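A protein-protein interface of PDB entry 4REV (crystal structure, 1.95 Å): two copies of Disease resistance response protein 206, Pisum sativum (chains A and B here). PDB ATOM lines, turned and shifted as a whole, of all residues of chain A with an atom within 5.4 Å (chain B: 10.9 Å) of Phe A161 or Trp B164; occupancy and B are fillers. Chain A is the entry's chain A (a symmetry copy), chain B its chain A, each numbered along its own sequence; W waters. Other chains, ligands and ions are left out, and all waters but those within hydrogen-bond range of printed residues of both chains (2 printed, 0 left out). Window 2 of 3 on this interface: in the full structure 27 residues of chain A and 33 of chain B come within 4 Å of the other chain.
CE2 of Phe B133 touches CD2 of Tyr A8, 3.8 Å away.
NH1 of Arg A136 touches CG of Arg B136, at 3.6 Å.
Gly B128 touches Ile A138 (O to CG2, 3.8 Å).
Ile A138 touches Phe B133.
Phe A161 touches Phe B133.
Met B134 touches Phe A161 (CE to CB, 3.8 Å).
Trp B164 touches Phe A161 (CH2 to O, 3.7 Å).
The guanidinium group of Arg A136 is in hydrogen-bond range of the backbone carbonyl oxygen of Met B134 (3.3 Å).
SD of Met B134 lies close to N of Gly A137 (3.7 Å).
The side-chain carboxylate of Glu B162 is in salt-bridge range of the guanidinium group of Arg A136, 2.6 Å away.
The chain-end carboxylate of Trp B164 lies within hydrogen-bond range of the side-chain hydroxyl of Tyr A8, 2.6 Å away.
SG of Cys B11 sits close to N of Glu B162 (3.7 Å).
The backbone carbonyl oxygen (O) of Phe B133 sits at hydrogen-bond distance from a ring nitrogen (ND1) of His B135, at 2.8 Å.
The backbone NH (N) of Phe B161 sits at hydrogen-bond distance from the backbone carbonyl oxygen (O) of Arg B136 (2.8 Å).
NH2 of Arg B136 is in salt-bridge range of OE1 of Glu B162 (2.9 Å).
NE1 of Trp B164 sits at hydrogen-bond distance from OE2 of Glu B162.
The side-chain sulfur (SG) of Cys A11 is disulfide-bonded to the side-chain sulfur (SG) of Cys A163 (2.1 Å).
Arg A136 touches its own counterpart, Arg B136.
Arg A136 touches Glu B162, but with the chains exchanged Glu A162 does not touch Arg B136 (5.7 Å).
8 positions are printed for both chains.
Of the 11 pairs that touch across the chains among the printed residues, 1 has its exchanged pair printed and touching as well.
Phe A161 touches just these residues of chain B: Phe B133, Met B134 and Trp B164.
No residue of chain B comes within 4 Å of Pro A10.
Gly A137 touches one residue of chain B.
Of chain B, only Gly B128 (3.8 Å) and Phe B133 (3.8 Å) come within 4 Å of Ile A138.
Of the printed residues of chain A, Met B134 touches Arg A136, Gly A137 and Phe A161.
Of the printed residues of chain A, Glu B162 touches Arg A136.
Cys A163 touches none of the printed residues of chain B.
Cys B11 touches none of the printed residues of chain A.
Of the 22 printed residues of chain B, 6 touch a printed residue of chain A.
Hydrophobic or aromatic side chains of chain B that line the printed part of chain A: Phe B133, Met B134 and Trp B164.
Hydrophobic or aromatic side chains of chain A within 4 Å of the printed part of chain B: Tyr A8, Ile A138 and Phe A161.
Water W2 lies within hydrogen-bond range of the backbone carbonyl oxygen (O) of Gly B128 (2.6 Å), the backbone NH (N) of Met B134 (2.9 Å) and the backbone carbonyl oxygen (O) of Gly A137 (3.1 Å).
Water W1 lies within hydrogen-bond range of NH2 of Arg B136 (2.9 Å), NH2 of Arg A136 (2.9 Å), OE1 of Glu A162 (3.1 Å) and OE1 of Glu B162 (3.1 Å).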
ATOM      1  N   TYR A   8      25.972  30.280  20.427  1.00  0.00           N
ATOM      2  CA  TYR A   8      27.266  30.371  21.093  1.00  0.00           C
ATOM      3  C   TYR A   8      28.422  30.339  20.094  1.00  0.00           C
ATOM      4  O   TYR A   8      28.359  29.630  19.085  1.00  0.00           O
ATOM      5  CB  TYR A   8      27.443  29.226  22.092  1.00  0.00           C
ATOM      6  CG  TYR A   8      26.315  29.037  23.075  1.00  0.00           C
ATOM      7  CD1 TYR A   8      26.316  29.677  24.304  1.00  0.00           C
ATOM      8  CD2 TYR A   8      25.242  28.218  22.763  1.00  0.00           C
ATOM      9  CE1 TYR A   8      25.289  29.479  25.203  1.00  0.00           C
ATOM     10  CE2 TYR A   8      24.216  28.020  23.647  1.00  0.00           C
ATOM     11  CZ  TYR A   8      24.242  28.644  24.864  1.00  0.00           C
ATOM     12  OH  TYR A   8      23.205  28.439  25.731  1.00  0.00           O
ATOM     13  N   LYS A   9      29.485  31.089  20.385  1.00  0.00           N
ATOM     14  CA  LYS A   9      30.697  31.010  19.574  1.00  0.00           C
ATOM     15  C   LYS A   9      31.753  30.163  20.290  1.00  0.00           C
ATOM     16  O   LYS A   9      32.054  30.381  21.461  1.00  0.00           O
ATOM     17  CB  LYS A   9      31.251  32.402  19.258  1.00  0.00           C
ATOM     18  CG  LYS A   9      32.691  32.382  18.764  1.00  0.00           C
ATOM     19  CD  LYS A   9      33.169  33.748  18.262  1.00  0.00           C
ATOM     20  CE  LYS A   9      34.689  33.750  18.066  1.00  0.00           C
ATOM     21  NZ  LYS A   9      35.326  35.064  18.371  1.00  0.00           N
ATOM     22  N   PRO A  10      32.322  29.192  19.579  1.00  0.00           N
ATOM     23  CA  PRO A  10      33.322  28.260  20.103  1.00  0.00           C
ATOM     24  C   PRO A  10      34.620  28.939  20.537  1.00  0.00           C
ATOM     25  O   PRO A  10      35.071  29.867  19.868  1.00  0.00           O
ATOM     26  CB  PRO A  10      33.581  27.316  18.918  1.00  0.00           C
ATOM     27  CG  PRO A  10      33.127  28.044  17.728  1.00  0.00           C
ATOM     28  CD  PRO A  10      32.007  28.940  18.161  1.00  0.00           C
ATOM     29  N   CYS A  11      35.212  28.480  21.635  1.00  0.00           N
ATOM     30  CA  CYS A  11      36.489  29.031  22.095  1.00  0.00           C
ATOM     31  C   CYS A  11      37.679  28.454  21.339  1.00  0.00           C
ATOM     32  O   CYS A  11      38.818  28.867  21.538  1.00  0.00           O
ATOM     33  CB  CYS A  11      36.652  28.817  23.605  1.00  0.00           C
ATOM     34  SG  CYS A  11      36.469  27.111  24.174  1.00  0.00           S
ATOM     35  N   ARG A 136      35.559  20.302  25.655  1.00  0.00           N
ATOM     36  CA  ARG A 136      34.216  19.800  25.362  1.00  0.00           C
ATOM     37  C   ARG A 136      33.616  20.517  24.174  1.00  0.00           C
ATOM     38  O   ARG A 136      33.960  21.645  23.879  1.00  0.00           O
ATOM     39  CB  ARG A 136      33.271  19.956  26.558  1.00  0.00           C
ATOM     40  CG  ARG A 136      33.611  19.016  27.698  1.00  0.00           C
ATOM     41  CD  ARG A 136      32.397  18.807  28.577  1.00  0.00           C
ATOM     42  NE  ARG A 136      32.048  20.009  29.263  1.00  0.00           N
ATOM     43  CZ  ARG A 136      30.840  20.556  29.350  1.00  0.00           C
ATOM     44  NH1 ARG A 136      29.730  20.036  28.815  1.00  0.00           N
ATOM     45  NH2 ARG A 136      30.758  21.656  30.029  1.00  0.00           N
ATOM     46  N   GLY A 137      32.687  19.847  23.504  1.00  0.00           N
ATOM     47  CA  GLY A 137      32.006  20.480  22.390  1.00  0.00           C
ATOM     48  C   GLY A 137      31.365  19.440  21.489  1.00  0.00           C
ATOM     49  O   GLY A 137      30.894  18.395  21.966  1.00  0.00           O
ATOM     50  N   ILE A 138      31.309  19.750  20.193  1.00  0.00           N
ATOM     51  CA  ILE A 138      30.720  18.834  19.211  1.00  0.00           C
ATOM     52  C   ILE A 138      31.578  18.820  17.967  1.00  0.00           C
ATOM     53  O   ILE A 138      32.385  19.733  17.749  1.00  0.00           O
ATOM     54  CB  ILE A 138      29.294  19.230  18.825  1.00  0.00           C
ATOM     55  CG1 ILE A 138      29.280  20.644  18.244  1.00  0.00           C
ATOM     56  CG2 ILE A 138      28.338  19.105  20.017  1.00  0.00           C
ATOM     57  CD1 ILE A 138      27.904  21.143  17.905  1.00  0.00           C
ATOM     58  N   LYS A 159      34.123  21.950  17.012  1.00  0.00           N
ATOM     59  CA  LYS A 159      33.847  23.214  17.673  1.00  0.00           C
ATOM     60  C   LYS A 159      33.872  22.947  19.166  1.00  0.00           C
ATOM     61  O   LYS A 159      32.985  22.264  19.684  1.00  0.00           O
ATOM     62  CB  LYS A 159      32.498  23.777  17.229  1.00  0.00           C
ATOM     63  CG  LYS A 159      32.517  24.385  15.846  1.00  0.00           C
ATOM     64  CD  LYS A 159      31.330  23.944  14.996  1.00  0.00           C
ATOM     65  CE  LYS A 159      31.476  22.487  14.556  1.00  0.00           C
ATOM     66  NZ  LYS A 159      30.368  22.034  13.673  1.00  0.00           N
ATOM     67  N   PHE A 160      34.901  23.443  19.852  1.00  0.00           N
ATOM     68  CA  PHE A 160      34.974  23.293  21.302  1.00  0.00           C
ATOM     69  C   PHE A 160      34.293  24.493  21.959  1.00  0.00           C
ATOM     70  O   PHE A 160      34.513  25.627  21.549  1.00  0.00           O
ATOM     71  CB  PHE A 160      36.424  23.195  21.800  1.00  0.00           C
ATOM     72  CG  PHE A 160      37.155  21.924  21.400  1.00  0.00           C
ATOM     73  CD1 PHE A 160      36.800  20.695  21.936  1.00  0.00           C
ATOM     74  CD2 PHE A 160      38.247  21.991  20.532  1.00  0.00           C
ATOM     75  CE1 PHE A 160      37.493  19.548  21.601  1.00  0.00           C
ATOM     76  CE2 PHE A 160      38.950  20.831  20.181  1.00  0.00           C
ATOM     77  CZ  PHE A 160      38.576  19.625  20.710  1.00  0.00           C
ATOM     78  N   PHE A 161      33.490  24.237  22.986  1.00  0.00           N
ATOM     79  CA  PHE A 161      32.825  25.306  23.714  1.00  0.00           C
ATOM     80  C   PHE A 161      33.313  25.387  25.149  1.00  0.00           C
ATOM     81  O   PHE A 161      32.867  26.233  25.930  1.00  0.00           O
ATOM     82  CB  PHE A 161      31.317  25.125  23.653  1.00  0.00           C
ATOM     83  CG  PHE A 161      30.759  25.423  22.305  1.00  0.00           C
ATOM     84  CD1 PHE A 161      30.803  24.466  21.301  1.00  0.00           C
ATOM     85  CD2 PHE A 161      30.236  26.663  22.015  1.00  0.00           C
ATOM     86  CE1 PHE A 161      30.295  24.748  20.037  1.00  0.00           C
ATOM     87  CE2 PHE A 161      29.738  26.945  20.756  1.00  0.00           C
ATOM     88  CZ  PHE A 161      29.776  25.984  19.769  1.00  0.00           C
ATOM     89  N   GLU A 162      34.234  24.494  25.485  1.00  0.00           N
ATOM     90  CA  GLU A 162      34.991  24.609  26.725  1.00  0.00           C
ATOM     91  C   GLU A 162      36.436  24.241  26.416  1.00  0.00           C
ATOM     92  O   GLU A 162      36.719  23.158  25.876  1.00  0.00           O
ATOM     93  CB  GLU A 162      34.426  23.720  27.837  1.00  0.00           C
ATOM     94  CG  GLU A 162      35.283  23.745  29.110  1.00  0.00           C
ATOM     95  CD  GLU A 162      34.682  22.965  30.276  1.00  0.00           C
ATOM     96  OE1 GLU A 162      33.471  22.685  30.254  1.00  0.00           O
ATOM     97  OE2 GLU A 162      35.421  22.658  31.233  1.00  0.00           O
ATOM     98  N   CYS A 163      37.342  25.169  26.721  1.00  0.00           N
ATOM     99  CA  CYS A 163      38.756  25.007  26.401  1.00  0.00           C
ATOM    100  C   CYS A 163      39.650  25.262  27.616  1.00  0.00           C
ATOM    101  O   CYS A 163      39.468  26.258  28.326  1.00  0.00           O
ATOM    102  CB  CYS A 163      39.147  25.967  25.264  1.00  0.00           C
ATOM    103  SG  CYS A 163      38.073  25.870  23.784  1.00  0.00           S
ATOM    104  N   PRO B  10      18.580  19.777  39.514  1.00  0.00           N
ATOM    105  CA  PRO B  10      18.841  19.750  38.073  1.00  0.00           C
ATOM    106  C   PRO B  10      18.274  20.958  37.328  1.00  0.00           C
ATOM    107  O   PRO B  10      17.177  21.408  37.652  1.00  0.00           O
ATOM    108  CB  PRO B  10      18.145  18.460  37.611  1.00  0.00           C
ATOM    109  CG  PRO B  10      17.170  18.142  38.660  1.00  0.00           C
ATOM    110  CD  PRO B  10      17.729  18.656  39.951  1.00  0.00           C
ATOM    111  N   CYS B  11      19.007  21.468  36.344  1.00  0.00           N
ATOM    112  CA  CYS B  11      18.519  22.590  35.538  1.00  0.00           C
ATOM    113  C   CYS B  11      17.553  22.146  34.446  1.00  0.00           C
ATOM    114  O   CYS B  11      16.983  22.966  33.732  1.00  0.00           O
ATOM    115  CB  CYS B  11      19.695  23.369  34.936  1.00  0.00           C
ATOM    116  SG  CYS B  11      20.875  22.384  33.983  1.00  0.00           S
ATOM    117  N   LYS B  12      17.368  20.836  34.321  1.00  0.00           N
ATOM    118  CA  LYS B  12      16.441  20.284  33.347  1.00  0.00           C
ATOM    119  C   LYS B  12      16.227  18.807  33.688  1.00  0.00           C
ATOM    120  O   LYS B  12      17.192  18.092  33.993  1.00  0.00           O
ATOM    121  CB  LYS B  12      16.974  20.475  31.914  1.00  0.00           C
ATOM    122  CG  LYS B  12      15.985  20.176  30.792  1.00  0.00           C
ATOM    123  CD  LYS B  12      16.639  20.303  29.392  1.00  0.00           C
ATOM    124  CE  LYS B  12      17.008  21.751  29.055  1.00  0.00           C
ATOM    125  NZ  LYS B  12      17.521  21.869  27.647  1.00  0.00           N
ATOM    126  N   LEU B  14      14.161  15.239  32.301  1.00  0.00           N
ATOM    127  CA  LEU B  14      13.404  14.591  31.235  1.00  0.00           C
ATOM    128  C   LEU B  14      13.126  13.137  31.582  1.00  0.00           C
ATOM    129  O   LEU B  14      13.946  12.465  32.217  1.00  0.00           O
ATOM    130  CB  LEU B  14      14.153  14.675  29.912  1.00  0.00           C
ATOM    131  CG  LEU B  14      14.292  16.071  29.299  1.00  0.00           C
ATOM    132  CD1 LEU B  14      15.005  15.959  27.969  1.00  0.00           C
ATOM    133  CD2 LEU B  14      12.926  16.730  29.129  1.00  0.00           C
ATOM    134  N   GLN B 105      14.737  17.930  19.781  1.00  0.00           N
ATOM    135  CA  GLN B 105      15.561  17.642  18.600  1.00  0.00           C
ATOM    136  C   GLN B 105      17.054  17.600  18.952  1.00  0.00           C
ATOM    137  O   GLN B 105      17.672  18.649  19.120  1.00  0.00           O
ATOM    138  CB  GLN B 105      15.330  18.704  17.528  1.00  0.00           C
ATOM    139  CG  GLN B 105      15.590  18.234  16.118  1.00  0.00           C
ATOM    140  CD  GLN B 105      14.371  17.573  15.503  1.00  0.00           C
ATOM    141  OE1 GLN B 105      13.283  17.589  16.081  1.00  0.00           O
ATOM    142  NE2 GLN B 105      14.545  16.993  14.323  1.00  0.00           N
ATOM    143  N   VAL B 125      25.496  10.653  31.775  1.00  0.00           N
ATOM    144  CA  VAL B 125      25.428  11.287  30.467  1.00  0.00           C
ATOM    145  C   VAL B 125      26.885  11.390  30.031  1.00  0.00           C
ATOM    146  O   VAL B 125      27.738  11.761  30.844  1.00  0.00           O
ATOM    147  CB  VAL B 125      24.765  12.692  30.529  1.00  0.00           C
ATOM    148  CG1 VAL B 125      24.992  13.459  29.183  1.00  0.00           C
ATOM    149  CG2 VAL B 125      23.254  12.585  30.847  1.00  0.00           C
ATOM    150  N   GLY B 127      27.562  12.426  26.504  1.00  0.00           N
ATOM    151  CA  GLY B 127      27.593  13.249  25.303  1.00  0.00           C
ATOM    152  C   GLY B 127      26.240  13.826  24.958  1.00  0.00           C
ATOM    153  O   GLY B 127      25.211  13.326  25.406  1.00  0.00           O
ATOM    154  N   GLY B 128      26.238  14.903  24.175  1.00  0.00           N
ATOM    155  CA  GLY B 128      25.000  15.560  23.803  1.00  0.00           C
ATOM    156  C   GLY B 128      25.178  16.305  22.482  1.00  0.00           C
ATOM    157  O   GLY B 128      26.268  16.832  22.200  1.00  0.00           O
ATOM    158  N   THR B 129      24.122  16.328  21.666  1.00  0.00           N
ATOM    159  CA  THR B 129      24.106  17.140  20.447  1.00  0.00           C
ATOM    160  C   THR B 129      22.749  17.821  20.237  1.00  0.00           C
ATOM    161  O   THR B 129      21.761  17.470  20.871  1.00  0.00           O
ATOM    162  CB  THR B 129      24.438  16.324  19.165  1.00  0.00           C
ATOM    163  OG1 THR B 129      23.381  15.403  18.873  1.00  0.00           O
ATOM    164  CG2 THR B 129      25.780  15.567  19.268  1.00  0.00           C
ATOM    165  N   GLY B 130      22.708  18.794  19.332  1.00  0.00           N
ATOM    166  CA  GLY B 130      21.467  19.477  18.998  1.00  0.00           C
ATOM    167  C   GLY B 130      20.945  20.236  20.206  1.00  0.00           C
ATOM    168  O   GLY B 130      21.685  20.990  20.829  1.00  0.00           O
ATOM    169  N   ASP B 131      19.668  20.033  20.539  1.00  0.00           N
ATOM    170  CA  ASP B 131      19.074  20.603  21.747  1.00  0.00           C
ATOM    171  C   ASP B 131      19.857  20.244  23.014  1.00  0.00           C
ATOM    172  O   ASP B 131      19.752  20.940  24.018  1.00  0.00           O
ATOM    173  CB  ASP B 131      17.616  20.129  21.924  1.00  0.00           C
ATOM    174  CG  ASP B 131      16.647  20.771  20.932  1.00  0.00           C
ATOM    175  OD1 ASP B 131      17.021  21.749  20.245  1.00  0.00           O
ATOM    176  OD2 ASP B 131      15.493  20.291  20.860  1.00  0.00           O
ATOM    177  N   PHE B 132      20.627  19.155  22.981  1.00  0.00           N
ATOM    178  CA  PHE B 132      21.335  18.706  24.185  1.00  0.00           C
ATOM    179  C   PHE B 132      22.836  18.885  24.132  1.00  0.00           C
ATOM    180  O   PHE B 132      23.570  18.351  24.953  1.00  0.00           O
ATOM    181  CB  PHE B 132      20.952  17.248  24.457  1.00  0.00           C
ATOM    182  CG  PHE B 132      19.476  17.075  24.504  1.00  0.00           C
ATOM    183  CD1 PHE B 132      18.770  17.555  25.600  1.00  0.00           C
ATOM    184  CD2 PHE B 132      18.780  16.504  23.446  1.00  0.00           C
ATOM    185  CE1 PHE B 132      17.381  17.456  25.654  1.00  0.00           C
ATOM    186  CE2 PHE B 132      17.391  16.395  23.493  1.00  0.00           C
ATOM    187  CZ  PHE B 132      16.693  16.868  24.603  1.00  0.00           C
ATOM    188  N   PHE B 133      23.261  19.613  23.112  1.00  0.00           N
ATOM    189  CA  PHE B 133      24.566  20.232  23.028  1.00  0.00           C
ATOM    190  C   PHE B 133      25.094  20.658  24.412  1.00  0.00           C
ATOM    191  O   PHE B 133      24.392  21.356  25.148  1.00  0.00           O
ATOM    192  CB  PHE B 133      24.407  21.429  22.068  1.00  0.00           C
ATOM    193  CG  PHE B 133      25.500  22.437  22.114  1.00  0.00           C
ATOM    194  CD1 PHE B 133      26.684  22.219  21.437  1.00  0.00           C
ATOM    195  CD2 PHE B 133      25.315  23.636  22.774  1.00  0.00           C
ATOM    196  CE1 PHE B 133      27.685  23.161  21.456  1.00  0.00           C
ATOM    197  CE2 PHE B 133      26.309  24.575  22.801  1.00  0.00           C
ATOM    198  CZ  PHE B 133      27.501  24.340  22.136  1.00  0.00           C
ATOM    199  N   MET B 134      26.300  20.196  24.758  1.00  0.00           N
ATOM    200  CA  MET B 134      27.005  20.543  25.988  1.00  0.00           C
ATOM    201  C   MET B 134      26.239  20.210  27.285  1.00  0.00           C
ATOM    202  O   MET B 134      26.580  20.718  28.358  1.00  0.00           O
ATOM    203  CB  MET B 134      27.361  22.049  25.984  1.00  0.00           C
ATOM    204  CG  MET B 134      28.387  22.393  24.892  1.00  0.00           C
ATOM    205  SD  MET B 134      30.042  21.754  25.253  1.00  0.00           S
ATOM    206  CE  MET B 134      30.517  22.881  26.592  1.00  0.00           C
ATOM    207  N   HIS B 135      25.192  19.393  27.196  1.00  0.00           N
ATOM    208  CA  HIS B 135      24.461  19.019  28.413  1.00  0.00           C
ATOM    209  C   HIS B 135      25.221  17.932  29.191  1.00  0.00           C
ATOM    210  O   HIS B 135      25.928  17.109  28.590  1.00  0.00           O
ATOM    211  CB  HIS B 135      23.043  18.512  28.105  1.00  0.00           C
ATOM    212  CG  HIS B 135      22.054  19.605  27.805  1.00  0.00           C
ATOM    213  ND1 HIS B 135      22.275  20.594  26.889  1.00  0.00           N
ATOM    214  CD2 HIS B 135      20.808  19.812  28.323  1.00  0.00           C
ATOM    215  CE1 HIS B 135      21.204  21.389  26.844  1.00  0.00           C
ATOM    216  NE2 HIS B 135      20.324  20.949  27.698  1.00  0.00           N
ATOM    217  N   ARG B 136      25.059  17.933  30.510  1.00  0.00           N
ATOM    218  CA  ARG B 136      25.691  16.922  31.358  1.00  0.00           C
ATOM    219  C   ARG B 136      24.794  16.545  32.515  1.00  0.00           C
ATOM    220  O   ARG B 136      23.967  17.322  32.948  1.00  0.00           O
ATOM    221  CB  ARG B 136      27.037  17.399  31.915  1.00  0.00           C
ATOM    222  CG  ARG B 136      28.111  17.493  30.848  1.00  0.00           C
ATOM    223  CD  ARG B 136      29.482  17.424  31.486  1.00  0.00           C
ATOM    224  NE  ARG B 136      29.736  18.581  32.281  1.00  0.00           N
ATOM    225  CZ  ARG B 136      30.201  18.607  33.526  1.00  0.00           C
ATOM    226  NH1 ARG B 136      30.535  17.524  34.235  1.00  0.00           N
ATOM    227  NH2 ARG B 136      30.355  19.780  34.054  1.00  0.00           N
ATOM    228  N   GLY B 137      24.990  15.337  33.028  1.00  0.00           N
ATOM    229  CA  GLY B 137      24.223  14.913  34.185  1.00  0.00           C
ATOM    230  C   GLY B 137      24.236  13.401  34.314  1.00  0.00           C
ATOM    231  O   GLY B 137      25.238  12.746  33.984  1.00  0.00           O
ATOM    232  N   PHE B 160      19.679  16.628  34.160  1.00  0.00           N
ATOM    233  CA  PHE B 160      20.829  17.388  33.679  1.00  0.00           C
ATOM    234  C   PHE B 160      21.227  18.411  34.743  1.00  0.00           C
ATOM    235  O   PHE B 160      20.369  19.080  35.306  1.00  0.00           O
ATOM    236  CB  PHE B 160      20.529  18.116  32.360  1.00  0.00           C
ATOM    237  CG  PHE B 160      20.333  17.209  31.157  1.00  0.00           C
ATOM    238  CD1 PHE B 160      21.392  16.495  30.618  1.00  0.00           C
ATOM    239  CD2 PHE B 160      19.085  17.137  30.533  1.00  0.00           C
ATOM    240  CE1 PHE B 160      21.219  15.702  29.500  1.00  0.00           C
ATOM    241  CE2 PHE B 160      18.899  16.330  29.404  1.00  0.00           C
ATOM    242  CZ  PHE B 160      19.954  15.622  28.894  1.00  0.00           C
ATOM    243  N   PHE B 161      22.526  18.537  34.994  1.00  0.00           N
ATOM    244  CA  PHE B 161      23.020  19.510  35.955  1.00  0.00           C
ATOM    245  C   PHE B 161      23.864  20.576  35.279  1.00  0.00           C
ATOM    246  O   PHE B 161      24.375  21.494  35.928  1.00  0.00           O
ATOM    247  CB  PHE B 161      23.795  18.811  37.060  1.00  0.00           C
ATOM    248  CG  PHE B 161      22.911  18.049  37.985  1.00  0.00           C
ATOM    249  CD1 PHE B 161      22.469  16.778  37.643  1.00  0.00           C
ATOM    250  CD2 PHE B 161      22.477  18.605  39.167  1.00  0.00           C
ATOM    251  CE1 PHE B 161      21.630  16.071  38.499  1.00  0.00           C
ATOM    252  CE2 PHE B 161      21.640  17.905  40.014  1.00  0.00           C
ATOM    253  CZ  PHE B 161      21.214  16.639  39.671  1.00  0.00           C
ATOM    254  N   GLU B 162      24.004  20.441  33.968  1.00  0.00           N
ATOM    255  CA  GLU B 162      24.548  21.514  33.144  1.00  0.00           C
ATOM    256  C   GLU B 162      23.724  21.573  31.865  1.00  0.00           C
ATOM    257  O   GLU B 162      23.571  20.564  31.154  1.00  0.00           O
ATOM    258  CB  GLU B 162      26.033  21.310  32.830  1.00  0.00           C
ATOM    259  CG  GLU B 162      26.587  22.370  31.868  1.00  0.00           C
ATOM    260  CD  GLU B 162      28.090  22.265  31.631  1.00  0.00           C
ATOM    261  OE1 GLU B 162      28.784  21.621  32.437  1.00  0.00           O
ATOM    262  OE2 GLU B 162      28.583  22.857  30.649  1.00  0.00           O
ATOM    263  N   CYS B 163      23.157  22.749  31.601  1.00  0.00           N
ATOM    264  CA  CYS B 163      22.263  22.943  30.465  1.00  0.00           C
ATOM    265  C   CYS B 163      22.666  24.151  29.619  1.00  0.00           C
ATOM    266  O   CYS B 163      22.933  25.230  30.160  1.00  0.00           O
ATOM    267  CB  CYS B 163      20.818  23.122  30.964  1.00  0.00           C
ATOM    268  SG  CYS B 163      20.238  21.813  32.104  1.00  0.00           S
ATOM    269  N   TRP B 164      22.691  23.981  28.299  1.00  0.00           N
ATOM    270  CA  TRP B 164      22.951  25.093  27.383  1.00  0.00           C
ATOM    271  C   TRP B 164      21.738  25.345  26.496  1.00  0.00           C
ATOM    272  O   TRP B 164      20.799  24.556  26.452  1.00  0.00           O
ATOM    273  CB  TRP B 164      24.177  24.827  26.509  1.00  0.00           C
ATOM    274  CG  TRP B 164      25.457  24.748  27.265  1.00  0.00           C
ATOM    275  CD1 TRP B 164      25.715  23.991  28.375  1.00  0.00           C
ATOM    276  CD2 TRP B 164      26.672  25.430  26.945  1.00  0.00           C
ATOM    277  NE1 TRP B 164      27.021  24.181  28.780  1.00  0.00           N
ATOM    278  CE2 TRP B 164      27.629  25.050  27.921  1.00  0.00           C
ATOM    279  CE3 TRP B 164      27.046  26.342  25.949  1.00  0.00           C
ATOM    280  CZ2 TRP B 164      28.932  25.561  27.922  1.00  0.00           C
ATOM    281  CZ3 TRP B 164      28.345  26.838  25.949  1.00  0.00           C
ATOM    282  CH2 TRP B 164      29.272  26.438  26.928  1.00  0.00           C
ATOM    283  OXT TRP B 164      21.668  26.346  25.803  1.00  0.00           O
HETATM  284  O   HOH W   1      31.825  21.965  32.750  1.00  0.00           O
HETATM  285  O   HOH W   2      28.029  18.446  23.245  1.00  0.00           O
